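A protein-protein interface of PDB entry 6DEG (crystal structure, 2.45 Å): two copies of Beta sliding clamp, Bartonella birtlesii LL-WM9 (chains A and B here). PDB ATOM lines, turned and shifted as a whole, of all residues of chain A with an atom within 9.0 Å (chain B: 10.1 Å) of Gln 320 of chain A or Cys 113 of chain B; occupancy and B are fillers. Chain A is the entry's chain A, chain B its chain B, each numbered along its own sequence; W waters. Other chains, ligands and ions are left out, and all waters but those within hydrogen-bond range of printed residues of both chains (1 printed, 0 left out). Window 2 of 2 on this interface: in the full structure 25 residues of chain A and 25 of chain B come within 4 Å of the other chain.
Gln 320 of chain A touches one residue of chain B. Cys 113 of chain B touches just these residues of chain A: Glu 318, Asp 319 and Gln 320. Of chain B, only Cys 113 and Thr 114 come within 4 Å of Asp 319 of chain A. No residue of chain B comes within 4 Å of Leu 321 of chain A. Of the printed residues of chain A, Phe 116 of chain B touches Arg 284 and Ala 317. Printed residues of chain A within 4 Å of Pro 90 of chain B: Arg 284. The nearest residue of chain B that does not touch Gln 320 of chain A is Thr 114 of chain B (5.4 Å).
Leu 89 of chain B touches Arg 284 of chain A. Arg 284 of chain A touches Pro 90 of chain B. O of Arg 284 of chain A touches CZ of Phe 116 of chain B, 3.4 Å away. Ala 317 of chain A touches His 115 of chain B. Ala 317 of chain A touches Phe 116 of chain B (CB to CE2, 3.5 Å). Glu 318 of chain A touches Cys 113 of chain B. Thr 114 of chain B touches Glu 318 of chain A. CB of Cys 113 of chain B touches O of Gln 320 of chain A, at 3.6 Å.
Hydrophobic or aromatic side chains of chain B that line the printed part of chain A: Leu 89, Pro 90, His 115 and Phe 116. Among the printed residues, 11 pairs touch across the chains. Among the printed residues, no Asp or Glu carboxylate lies within 4 Å of a Lys or Arg side-chain nitrogen of the other chain.
The backbone carbonyl oxygen (O) of Asp 319 of chain A lies within hydrogen-bond range of the backbone NH (N) of Leu 307 of chain A. The side-chain hydroxyl (OG) of Ser 93 of chain B sits at hydrogen-bond distance from the backbone carbonyl oxygen (O) of Pro 90 of chain B (2.8 Å). The backbone NH (N) of Phe 116 of chain B sits at hydrogen-bond distance from the backbone carbonyl oxygen (O) of Ile 109 of chain B, at 3.0 Å. The backbone carbonyl oxygen (O) of Ser 111 of chain B sits at hydrogen-bond distance from the side-chain hydroxyl (OG1) of Thr 114 of chain B (3.0 Å).
No position is printed for both chains. Of the 11 pairs that touch across the chains among the printed residues, none has its exchanged pair printed and touching as well.
The backbone NH (N) of Glu 318 of chain A sits at hydrogen-bond distance from the backbone carbonyl oxygen (O) of His 115 of chain B, at 2.6 Å. The side-chain carboxylate (OD2) of Asp 319 of chain A sits at hydrogen-bond distance from the side-chain hydroxyl (OG1) of Thr 114 of chain B (3.5 Å). The side-chain carboxylate (OD1) of Asp 319 of chain A lies close to the backbone carbonyl oxygen (O) of Cys 113 of chain B, 3.2 Å away.
Water W1 lies within hydrogen-bond range of NE of Arg 284 of chain A and OG1 of Thr 114 of chain B.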
ATOM      1  N   VAL A 273     -31.841  22.179  30.862  1.00  0.00           N
ATOM      2  CA  VAL A 273     -31.278  20.901  30.452  1.00  0.00           C
ATOM      3  C   VAL A 273     -30.686  20.237  31.686  1.00  0.00           C
ATOM      4  O   VAL A 273     -30.339  20.897  32.667  1.00  0.00           O
ATOM      5  CB  VAL A 273     -30.190  21.043  29.363  1.00  0.00           C
ATOM      6  CG1 VAL A 273     -30.798  21.465  28.038  1.00  0.00           C
ATOM      7  CG2 VAL A 273     -29.127  22.033  29.809  1.00  0.00           C
ATOM      8  N   ASP A 277     -25.981  15.531  32.063  1.00  0.00           N
ATOM      9  CA  ASP A 277     -26.111  15.152  30.661  1.00  0.00           C
ATOM     10  C   ASP A 277     -25.532  16.221  29.746  1.00  0.00           C
ATOM     11  O   ASP A 277     -25.033  15.911  28.660  1.00  0.00           O
ATOM     12  CB  ASP A 277     -27.578  14.900  30.318  1.00  0.00           C
ATOM     13  CG  ASP A 277     -28.192  13.803  31.159  1.00  0.00           C
ATOM     14  OD1 ASP A 277     -27.636  13.496  32.235  1.00  0.00           O
ATOM     15  OD2 ASP A 277     -29.230  13.248  30.749  1.00  0.00           O
ATOM     16  N   PHE A 278     -25.597  17.483  30.165  1.00  0.00           N
ATOM     17  CA  PHE A 278     -25.142  18.580  29.323  1.00  0.00           C
ATOM     18  C   PHE A 278     -23.625  18.699  29.331  1.00  0.00           C
ATOM     19  O   PHE A 278     -23.002  18.845  28.275  1.00  0.00           O
ATOM     20  CB  PHE A 278     -25.786  19.886  29.783  1.00  0.00           C
ATOM     21  CG  PHE A 278     -25.315  21.082  29.030  1.00  0.00           C
ATOM     22  CD1 PHE A 278     -25.701  21.281  27.717  1.00  0.00           C
ATOM     23  CD2 PHE A 278     -24.483  22.011  29.631  1.00  0.00           C
ATOM     24  CE1 PHE A 278     -25.267  22.389  27.013  1.00  0.00           C
ATOM     25  CE2 PHE A 278     -24.044  23.121  28.938  1.00  0.00           C
ATOM     26  CZ  PHE A 278     -24.436  23.312  27.627  1.00  0.00           C
ATOM     27  N   ALA A 281     -22.122  15.896  27.303  1.00  0.00           N
ATOM     28  CA  ALA A 281     -22.347  16.108  25.876  1.00  0.00           C
ATOM     29  C   ALA A 281     -21.424  17.187  25.320  1.00  0.00           C
ATOM     30  O   ALA A 281     -20.859  17.031  24.233  1.00  0.00           O
ATOM     31  CB  ALA A 281     -23.809  16.475  25.627  1.00  0.00           C
ATOM     32  N   VAL A 282     -21.263  18.289  26.051  1.00  0.00           N
ATOM     33  CA  VAL A 282     -20.338  19.337  25.626  1.00  0.00           C
ATOM     34  C   VAL A 282     -18.911  18.806  25.596  1.00  0.00           C
ATOM     35  O   VAL A 282     -18.110  19.170  24.725  1.00  0.00           O
ATOM     36  CB  VAL A 282     -20.466  20.561  26.549  1.00  0.00           C
ATOM     37  CG1 VAL A 282     -19.378  21.578  26.247  1.00  0.00           C
ATOM     38  CG2 VAL A 282     -21.841  21.184  26.407  1.00  0.00           C
ATOM     39  N   ARG A 284     -17.860  15.850  24.810  1.00  0.00           N
ATOM     40  CA  ARG A 284     -17.579  14.929  23.715  1.00  0.00           C
ATOM     41  C   ARG A 284     -17.356  15.656  22.390  1.00  0.00           C
ATOM     42  O   ARG A 284     -16.399  15.357  21.666  1.00  0.00           O
ATOM     43  CB  ARG A 284     -18.716  13.912  23.616  1.00  0.00           C
ATOM     44  CG  ARG A 284     -18.828  13.049  24.871  1.00  0.00           C
ATOM     45  CD  ARG A 284     -19.995  12.072  24.836  1.00  0.00           C
ATOM     46  NE  ARG A 284     -20.008  11.209  26.018  1.00  0.00           N
ATOM     47  CZ  ARG A 284     -20.919  11.267  26.985  1.00  0.00           C
ATOM     48  NH1 ARG A 284     -21.911  12.145  26.917  1.00  0.00           N
ATOM     49  NH2 ARG A 284     -20.841  10.442  28.021  1.00  0.00           N
ATOM     50  N   VAL A 285     -18.216  16.625  22.059  1.00  0.00           N
ATOM     51  CA  VAL A 285     -18.149  17.262  20.742  1.00  0.00           C
ATOM     52  C   VAL A 285     -16.977  18.227  20.588  1.00  0.00           C
ATOM     53  O   VAL A 285     -16.551  18.490  19.458  1.00  0.00           O
ATOM     54  CB  VAL A 285     -19.468  17.995  20.421  1.00  0.00           C
ATOM     55  CG1 VAL A 285     -20.579  17.004  20.136  1.00  0.00           C
ATOM     56  CG2 VAL A 285     -19.861  18.918  21.566  1.00  0.00           C
ATOM     57  N   THR A 299     -27.975  24.638  18.586  1.00  0.00           N
ATOM     58  CA  THR A 299     -29.201  24.793  17.817  1.00  0.00           C
ATOM     59  C   THR A 299     -30.378  24.441  18.718  1.00  0.00           C
ATOM     60  O   THR A 299     -30.503  23.295  19.163  1.00  0.00           O
ATOM     61  CB  THR A 299     -29.183  23.908  16.576  1.00  0.00           C
ATOM     62  OG1 THR A 299     -28.077  24.282  15.745  1.00  0.00           O
ATOM     63  CG2 THR A 299     -30.475  24.079  15.793  1.00  0.00           C
ATOM     64  N   GLU A 301     -34.407  24.206  19.542  1.00  0.00           N
ATOM     65  CA  GLU A 301     -35.782  24.054  19.086  1.00  0.00           C
ATOM     66  C   GLU A 301     -36.659  23.751  20.297  1.00  0.00           C
ATOM     67  O   GLU A 301     -36.195  23.749  21.439  1.00  0.00           O
ATOM     68  CB  GLU A 301     -35.898  22.957  18.020  1.00  0.00           C
ATOM     69  N   HIS A 302     -37.942  23.493  20.046  1.00  0.00           N
ATOM     70  CA  HIS A 302     -38.895  23.230  21.122  1.00  0.00           C
ATOM     71  C   HIS A 302     -38.632  21.867  21.750  1.00  0.00           C
ATOM     72  O   HIS A 302     -38.857  20.828  21.123  1.00  0.00           O
ATOM     73  CB  HIS A 302     -40.323  23.315  20.594  1.00  0.00           C
ATOM     74  CG  HIS A 302     -40.845  24.712  20.511  1.00  0.00           C
ATOM     75  ND1 HIS A 302     -41.994  25.115  21.155  1.00  0.00           N
ATOM     76  CD2 HIS A 302     -40.365  25.805  19.874  1.00  0.00           C
ATOM     77  CE1 HIS A 302     -42.208  26.395  20.909  1.00  0.00           C
ATOM     78  NE2 HIS A 302     -41.234  26.837  20.134  1.00  0.00           N
ATOM     79  N   GLY A 303     -38.167  21.871  22.995  1.00  0.00           N
ATOM     80  CA  GLY A 303     -37.916  20.635  23.711  1.00  0.00           C
ATOM     81  C   GLY A 303     -36.827  19.764  23.132  1.00  0.00           C
ATOM     82  O   GLY A 303     -36.813  18.556  23.384  1.00  0.00           O
ATOM     83  N   GLN A 304     -35.900  20.342  22.374  1.00  0.00           N
ATOM     84  CA  GLN A 304     -34.816  19.586  21.763  1.00  0.00           C
ATOM     85  C   GLN A 304     -33.585  20.472  21.701  1.00  0.00           C
ATOM     86  O   GLN A 304     -33.692  21.701  21.680  1.00  0.00           O
ATOM     87  CB  GLN A 304     -35.189  19.082  20.359  1.00  0.00           C
ATOM     88  N   LEU A 305     -32.414  19.838  21.696  1.00  0.00           N
ATOM     89  CA  LEU A 305     -31.156  20.578  21.704  1.00  0.00           C
ATOM     90  C   LEU A 305     -30.133  19.807  20.881  1.00  0.00           C
ATOM     91  O   LEU A 305     -29.695  18.730  21.295  1.00  0.00           O
ATOM     92  CB  LEU A 305     -30.666  20.786  23.131  1.00  0.00           C
ATOM     93  CG  LEU A 305     -29.361  21.558  23.331  1.00  0.00           C
ATOM     94  CD1 LEU A 305     -29.165  22.686  22.306  1.00  0.00           C
ATOM     95  CD2 LEU A 305     -29.294  22.087  24.756  1.00  0.00           C
ATOM     96  N   LYS A 306     -29.745  20.362  19.731  1.00  0.00           N
ATOM     97  CA  LYS A 306     -28.705  19.779  18.898  1.00  0.00           C
ATOM     98  C   LYS A 306     -27.421  20.566  19.099  1.00  0.00           C
ATOM     99  O   LYS A 306     -27.439  21.800  19.078  1.00  0.00           O
ATOM    100  CB  LYS A 306     -29.116  19.785  17.428  1.00  0.00           C
ATOM    101  N   LEU A 307     -26.319  19.851  19.310  1.00  0.00           N
ATOM    102  CA  LEU A 307     -24.996  20.440  19.484  1.00  0.00           C
ATOM    103  C   LEU A 307     -24.141  20.217  18.245  1.00  0.00           C
ATOM    104  O   LEU A 307     -24.150  19.128  17.666  1.00  0.00           O
ATOM    105  CB  LEU A 307     -24.292  19.856  20.710  1.00  0.00           C
ATOM    106  CG  LEU A 307     -25.007  20.141  22.025  1.00  0.00           C
ATOM    107  CD1 LEU A 307     -24.441  19.305  23.169  1.00  0.00           C
ATOM    108  CD2 LEU A 307     -24.929  21.627  22.331  1.00  0.00           C
ATOM    109  N   VAL A 308     -23.400  21.247  17.841  1.00  0.00           N
ATOM    110  CA  VAL A 308     -22.693  21.239  16.564  1.00  0.00           C
ATOM    111  C   VAL A 308     -21.313  21.862  16.759  1.00  0.00           C
ATOM    112  O   VAL A 308     -21.204  23.049  17.077  1.00  0.00           O
ATOM    113  CB  VAL A 308     -23.461  21.998  15.468  1.00  0.00           C
ATOM    114  CG1 VAL A 308     -22.611  22.128  14.221  1.00  0.00           C
ATOM    115  CG2 VAL A 308     -24.781  21.330  15.158  1.00  0.00           C
ATOM    116  N   ALA A 317     -19.037  17.233  14.349  1.00  0.00           N
ATOM    117  CA  ALA A 317     -19.570  16.463  15.461  1.00  0.00           C
ATOM    118  C   ALA A 317     -21.018  16.864  15.706  1.00  0.00           C
ATOM    119  O   ALA A 317     -21.453  17.961  15.349  1.00  0.00           O
ATOM    120  CB  ALA A 317     -18.746  16.661  16.737  1.00  0.00           C
ATOM    121  N   GLU A 318     -21.767  15.950  16.319  1.00  0.00           N
ATOM    122  CA  GLU A 318     -23.184  16.161  16.571  1.00  0.00           C
ATOM    123  C   GLU A 318     -23.598  15.451  17.849  1.00  0.00           C
ATOM    124  O   GLU A 318     -23.116  14.354  18.139  1.00  0.00           O
ATOM    125  CB  GLU A 318     -24.042  15.648  15.416  1.00  0.00           C
ATOM    126  CG  GLU A 318     -24.324  16.661  14.345  1.00  0.00           C
ATOM    127  CD  GLU A 318     -25.734  16.529  13.822  1.00  0.00           C
ATOM    128  OE1 GLU A 318     -25.911  15.929  12.741  1.00  0.00           O
ATOM    129  OE2 GLU A 318     -26.665  17.012  14.503  1.00  0.00           O
ATOM    130  N   ASP A 319     -24.493  16.083  18.602  1.00  0.00           N
ATOM    131  CA  ASP A 319     -25.169  15.415  19.703  1.00  0.00           C
ATOM    132  C   ASP A 319     -26.524  16.077  19.914  1.00  0.00           C
ATOM    133  O   ASP A 319     -26.764  17.201  19.469  1.00  0.00           O
ATOM    134  CB  ASP A 319     -24.343  15.446  20.989  1.00  0.00           C
ATOM    135  CG  ASP A 319     -24.723  14.335  21.943  1.00  0.00           C
ATOM    136  OD1 ASP A 319     -25.747  13.668  21.689  1.00  0.00           O
ATOM    137  OD2 ASP A 319     -24.006  14.127  22.943  1.00  0.00           O
ATOM    138  N   GLN A 320     -27.408  15.364  20.603  1.00  0.00           N
ATOM    139  CA  GLN A 320     -28.756  15.850  20.839  1.00  0.00           C
ATOM    140  C   GLN A 320     -29.221  15.440  22.227  1.00  0.00           C
ATOM    141  O   GLN A 320     -28.988  14.306  22.656  1.00  0.00           O
ATOM    142  CB  GLN A 320     -29.716  15.303  19.775  1.00  0.00           C
ATOM    143  CG  GLN A 320     -31.132  15.829  19.870  1.00  0.00           C
ATOM    144  CD  GLN A 320     -31.929  15.553  18.615  1.00  0.00           C
ATOM    145  OE1 GLN A 320     -31.517  14.763  17.765  1.00  0.00           O
ATOM    146  NE2 GLN A 320     -33.075  16.213  18.485  1.00  0.00           N
ATOM    147  N   LEU A 321     -29.866  16.366  22.933  1.00  0.00           N
ATOM    148  CA  LEU A 321     -30.458  16.064  24.228  1.00  0.00           C
ATOM    149  C   LEU A 321     -31.802  16.770  24.353  1.00  0.00           C
ATOM    150  O   LEU A 321     -32.160  17.635  23.548  1.00  0.00           O
ATOM    151  CB  LEU A 321     -29.532  16.430  25.394  1.00  0.00           C
ATOM    152  CG  LEU A 321     -28.947  17.830  25.523  1.00  0.00           C
ATOM    153  CD1 LEU A 321     -28.695  18.127  26.988  1.00  0.00           C
ATOM    154  CD2 LEU A 321     -27.660  17.919  24.734  1.00  0.00           C
ATOM    155  N   ALA A 322     -32.556  16.366  25.373  1.00  0.00           N
ATOM    156  CA  ALA A 322     -33.865  16.940  25.653  1.00  0.00           C
ATOM    157  C   ALA A 322     -33.736  18.209  26.486  1.00  0.00           C
ATOM    158  O   ALA A 322     -33.024  18.234  27.495  1.00  0.00           O
ATOM    159  CB  ALA A 322     -34.747  15.925  26.378  1.00  0.00           C
ATOM    160  N   ALA A 323     -34.434  19.257  26.066  1.00  0.00           N
ATOM    161  CA  ALA A 323     -34.361  20.556  26.709  1.00  0.00           C
ATOM    162  C   ALA A 323     -35.763  21.024  27.073  1.00  0.00           C
ATOM    163  O   ALA A 323     -36.762  20.524  26.550  1.00  0.00           O
ATOM    164  CB  ALA A 323     -33.680  21.585  25.803  1.00  0.00           C
ATOM    165  N   LEU B  89     -15.668   9.049  25.641  1.00  0.00           N
ATOM    166  CA  LEU B  89     -16.927   8.339  25.475  1.00  0.00           C
ATOM    167  C   LEU B  89     -17.178   7.427  26.673  1.00  0.00           C
ATOM    168  O   LEU B  89     -16.233   6.855  27.224  1.00  0.00           O
ATOM    169  CB  LEU B  89     -16.929   7.525  24.185  1.00  0.00           C
ATOM    170  CG  LEU B  89     -17.282   8.333  22.939  1.00  0.00           C
ATOM    171  CD1 LEU B  89     -17.384   7.427  21.725  1.00  0.00           C
ATOM    172  CD2 LEU B  89     -18.572   9.114  23.148  1.00  0.00           C
ATOM    173  N   PRO B  90     -18.434   7.274  27.098  1.00  0.00           N
ATOM    174  CA  PRO B  90     -18.713   6.497  28.312  1.00  0.00           C
ATOM    175  C   PRO B  90     -18.146   5.089  28.220  1.00  0.00           C
ATOM    176  O   PRO B  90     -18.200   4.440  27.173  1.00  0.00           O
ATOM    177  CB  PRO B  90     -20.245   6.487  28.391  1.00  0.00           C
ATOM    178  CG  PRO B  90     -20.725   6.927  27.044  1.00  0.00           C
ATOM    179  CD  PRO B  90     -19.661   7.815  26.491  1.00  0.00           C
ATOM    180  N   SER B  93     -19.473   1.394  26.624  1.00  0.00           N
ATOM    181  CA  SER B  93     -20.420   1.624  25.549  1.00  0.00           C
ATOM    182  C   SER B  93     -19.967   0.900  24.284  1.00  0.00           C
ATOM    183  O   SER B  93     -18.861   0.358  24.198  1.00  0.00           O
ATOM    184  CB  SER B  93     -20.570   3.120  25.274  1.00  0.00           C
ATOM    185  OG  SER B  93     -19.368   3.665  24.759  1.00  0.00           O
ATOM    186  N   GLU B  94     -20.842   0.896  23.288  1.00  0.00           N
ATOM    187  CA  GLU B  94     -20.550   0.309  21.991  1.00  0.00           C
ATOM    188  C   GLU B  94     -20.523   1.419  20.955  1.00  0.00           C
ATOM    189  O   GLU B  94     -21.413   2.277  20.934  1.00  0.00           O
ATOM    190  CB  GLU B  94     -21.576  -0.763  21.623  1.00  0.00           C
ATOM    191  CG  GLU B  94     -21.365  -2.070  22.363  1.00  0.00           C
ATOM    192  CD  GLU B  94     -21.870  -3.265  21.590  1.00  0.00           C
ATOM    193  OE1 GLU B  94     -22.829  -3.105  20.806  1.00  0.00           O
ATOM    194  OE2 GLU B  94     -21.303  -4.363  21.765  1.00  0.00           O
ATOM    195  N   ILE B 109     -18.978   8.071  12.912  1.00  0.00           N
ATOM    196  CA  ILE B 109     -18.935   7.482  14.246  1.00  0.00           C
ATOM    197  C   ILE B 109     -20.277   7.724  14.924  1.00  0.00           C
ATOM    198  O   ILE B 109     -20.853   8.811  14.802  1.00  0.00           O
ATOM    199  CB  ILE B 109     -17.785   8.072  15.084  1.00  0.00           C
ATOM    200  CG1 ILE B 109     -16.490   8.074  14.275  1.00  0.00           C
ATOM    201  CG2 ILE B 109     -17.607   7.292  16.372  1.00  0.00           C
ATOM    202  CD1 ILE B 109     -15.377   8.852  14.931  1.00  0.00           C
ATOM    203  N   VAL B 110     -20.780   6.711  15.632  1.00  0.00           N
ATOM    204  CA  VAL B 110     -22.083   6.790  16.287  1.00  0.00           C
ATOM    205  C   VAL B 110     -21.973   6.159  17.668  1.00  0.00           C
ATOM    206  O   VAL B 110     -21.665   4.968  17.785  1.00  0.00           O
ATOM    207  CB  VAL B 110     -23.190   6.088  15.479  1.00  0.00           C
ATOM    208  CG1 VAL B 110     -24.458   5.962  16.311  1.00  0.00           C
ATOM    209  CG2 VAL B 110     -23.465   6.836  14.183  1.00  0.00           C
ATOM    210  N   SER B 111     -22.217   6.950  18.710  1.00  0.00           N
ATOM    211  CA  SER B 111     -22.369   6.425  20.065  1.00  0.00           C
ATOM    212  C   SER B 111     -23.576   7.126  20.683  1.00  0.00           C
ATOM    213  O   SER B 111     -23.483   8.289  21.085  1.00  0.00           O
ATOM    214  CB  SER B 111     -21.108   6.637  20.894  1.00  0.00           C
ATOM    215  OG  SER B 111     -21.035   5.707  21.963  1.00  0.00           O
ATOM    216  N   GLY B 112     -24.699   6.421  20.756  1.00  0.00           N
ATOM    217  CA  GLY B 112     -25.917   7.060  21.222  1.00  0.00           C
ATOM    218  C   GLY B 112     -26.332   8.157  20.267  1.00  0.00           C
ATOM    219  O   GLY B 112     -26.334   7.982  19.044  1.00  0.00           O
ATOM    220  N   CYS B 113     -26.688   9.309  20.827  1.00  0.00           N
ATOM    221  CA  CYS B 113     -27.033  10.471  20.021  1.00  0.00           C
ATOM    222  C   CYS B 113     -25.809  11.258  19.575  1.00  0.00           C
ATOM    223  O   CYS B 113     -25.962  12.264  18.872  1.00  0.00           O
ATOM    224  CB  CYS B 113     -27.992  11.382  20.791  1.00  0.00           C
ATOM    225  SG  CYS B 113     -29.733  10.936  20.594  1.00  0.00           S
ATOM    226  N   THR B 114     -24.611  10.835  19.976  1.00  0.00           N
ATOM    227  CA  THR B 114     -23.382  11.453  19.497  1.00  0.00           C
ATOM    228  C   THR B 114     -23.059  10.946  18.098  1.00  0.00           C
ATOM    229  O   THR B 114     -23.191   9.754  17.808  1.00  0.00           O
ATOM    230  CB  THR B 114     -22.213  11.152  20.436  1.00  0.00           C
ATOM    231  OG1 THR B 114     -22.671  11.128  21.792  1.00  0.00           O
ATOM    232  CG2 THR B 114     -21.143  12.216  20.298  1.00  0.00           C
ATOM    233  N   HIS B 115     -22.625  11.857  17.232  1.00  0.00           N
ATOM    234  CA  HIS B 115     -22.340  11.518  15.843  1.00  0.00           C
ATOM    235  C   HIS B 115     -21.156  12.346  15.370  1.00  0.00           C
ATOM    236  O   HIS B 115     -21.190  13.577  15.449  1.00  0.00           O
ATOM    237  CB  HIS B 115     -23.567  11.766  14.959  1.00  0.00           C
ATOM    238  CG  HIS B 115     -23.240  12.041  13.524  1.00  0.00           C
ATOM    239  ND1 HIS B 115     -23.147  13.318  13.013  1.00  0.00           N
ATOM    240  CD2 HIS B 115     -22.993  11.202  12.491  1.00  0.00           C
ATOM    241  CE1 HIS B 115     -22.853  13.254  11.727  1.00  0.00           C
ATOM    242  NE2 HIS B 115     -22.754  11.981  11.384  1.00  0.00           N
ATOM    243  N   PHE B 116     -20.118  11.673  14.885  1.00  0.00           N
ATOM    244  CA  PHE B 116     -18.947  12.329  14.324  1.00  0.00           C
ATOM    245  C   PHE B 116     -18.832  12.021  12.838  1.00  0.00           C
ATOM    246  O   PHE B 116     -19.456  11.094  12.317  1.00  0.00           O
ATOM    247  CB  PHE B 116     -17.658  11.887  15.029  1.00  0.00           C
ATOM    248  CG  PHE B 116     -17.497  12.427  16.423  1.00  0.00           C
ATOM    249  CD1 PHE B 116     -18.053  11.769  17.506  1.00  0.00           C
ATOM    250  CD2 PHE B 116     -16.775  13.585  16.650  1.00  0.00           C
ATOM    251  CE1 PHE B 116     -17.900  12.264  18.793  1.00  0.00           C
ATOM    252  CE2 PHE B 116     -16.619  14.085  17.934  1.00  0.00           C
ATOM    253  CZ  PHE B 116     -17.182  13.423  19.005  1.00  0.00           C
HETATM  254  O   HOH W   1     -21.900   9.466  24.460  1.00  0.00           O
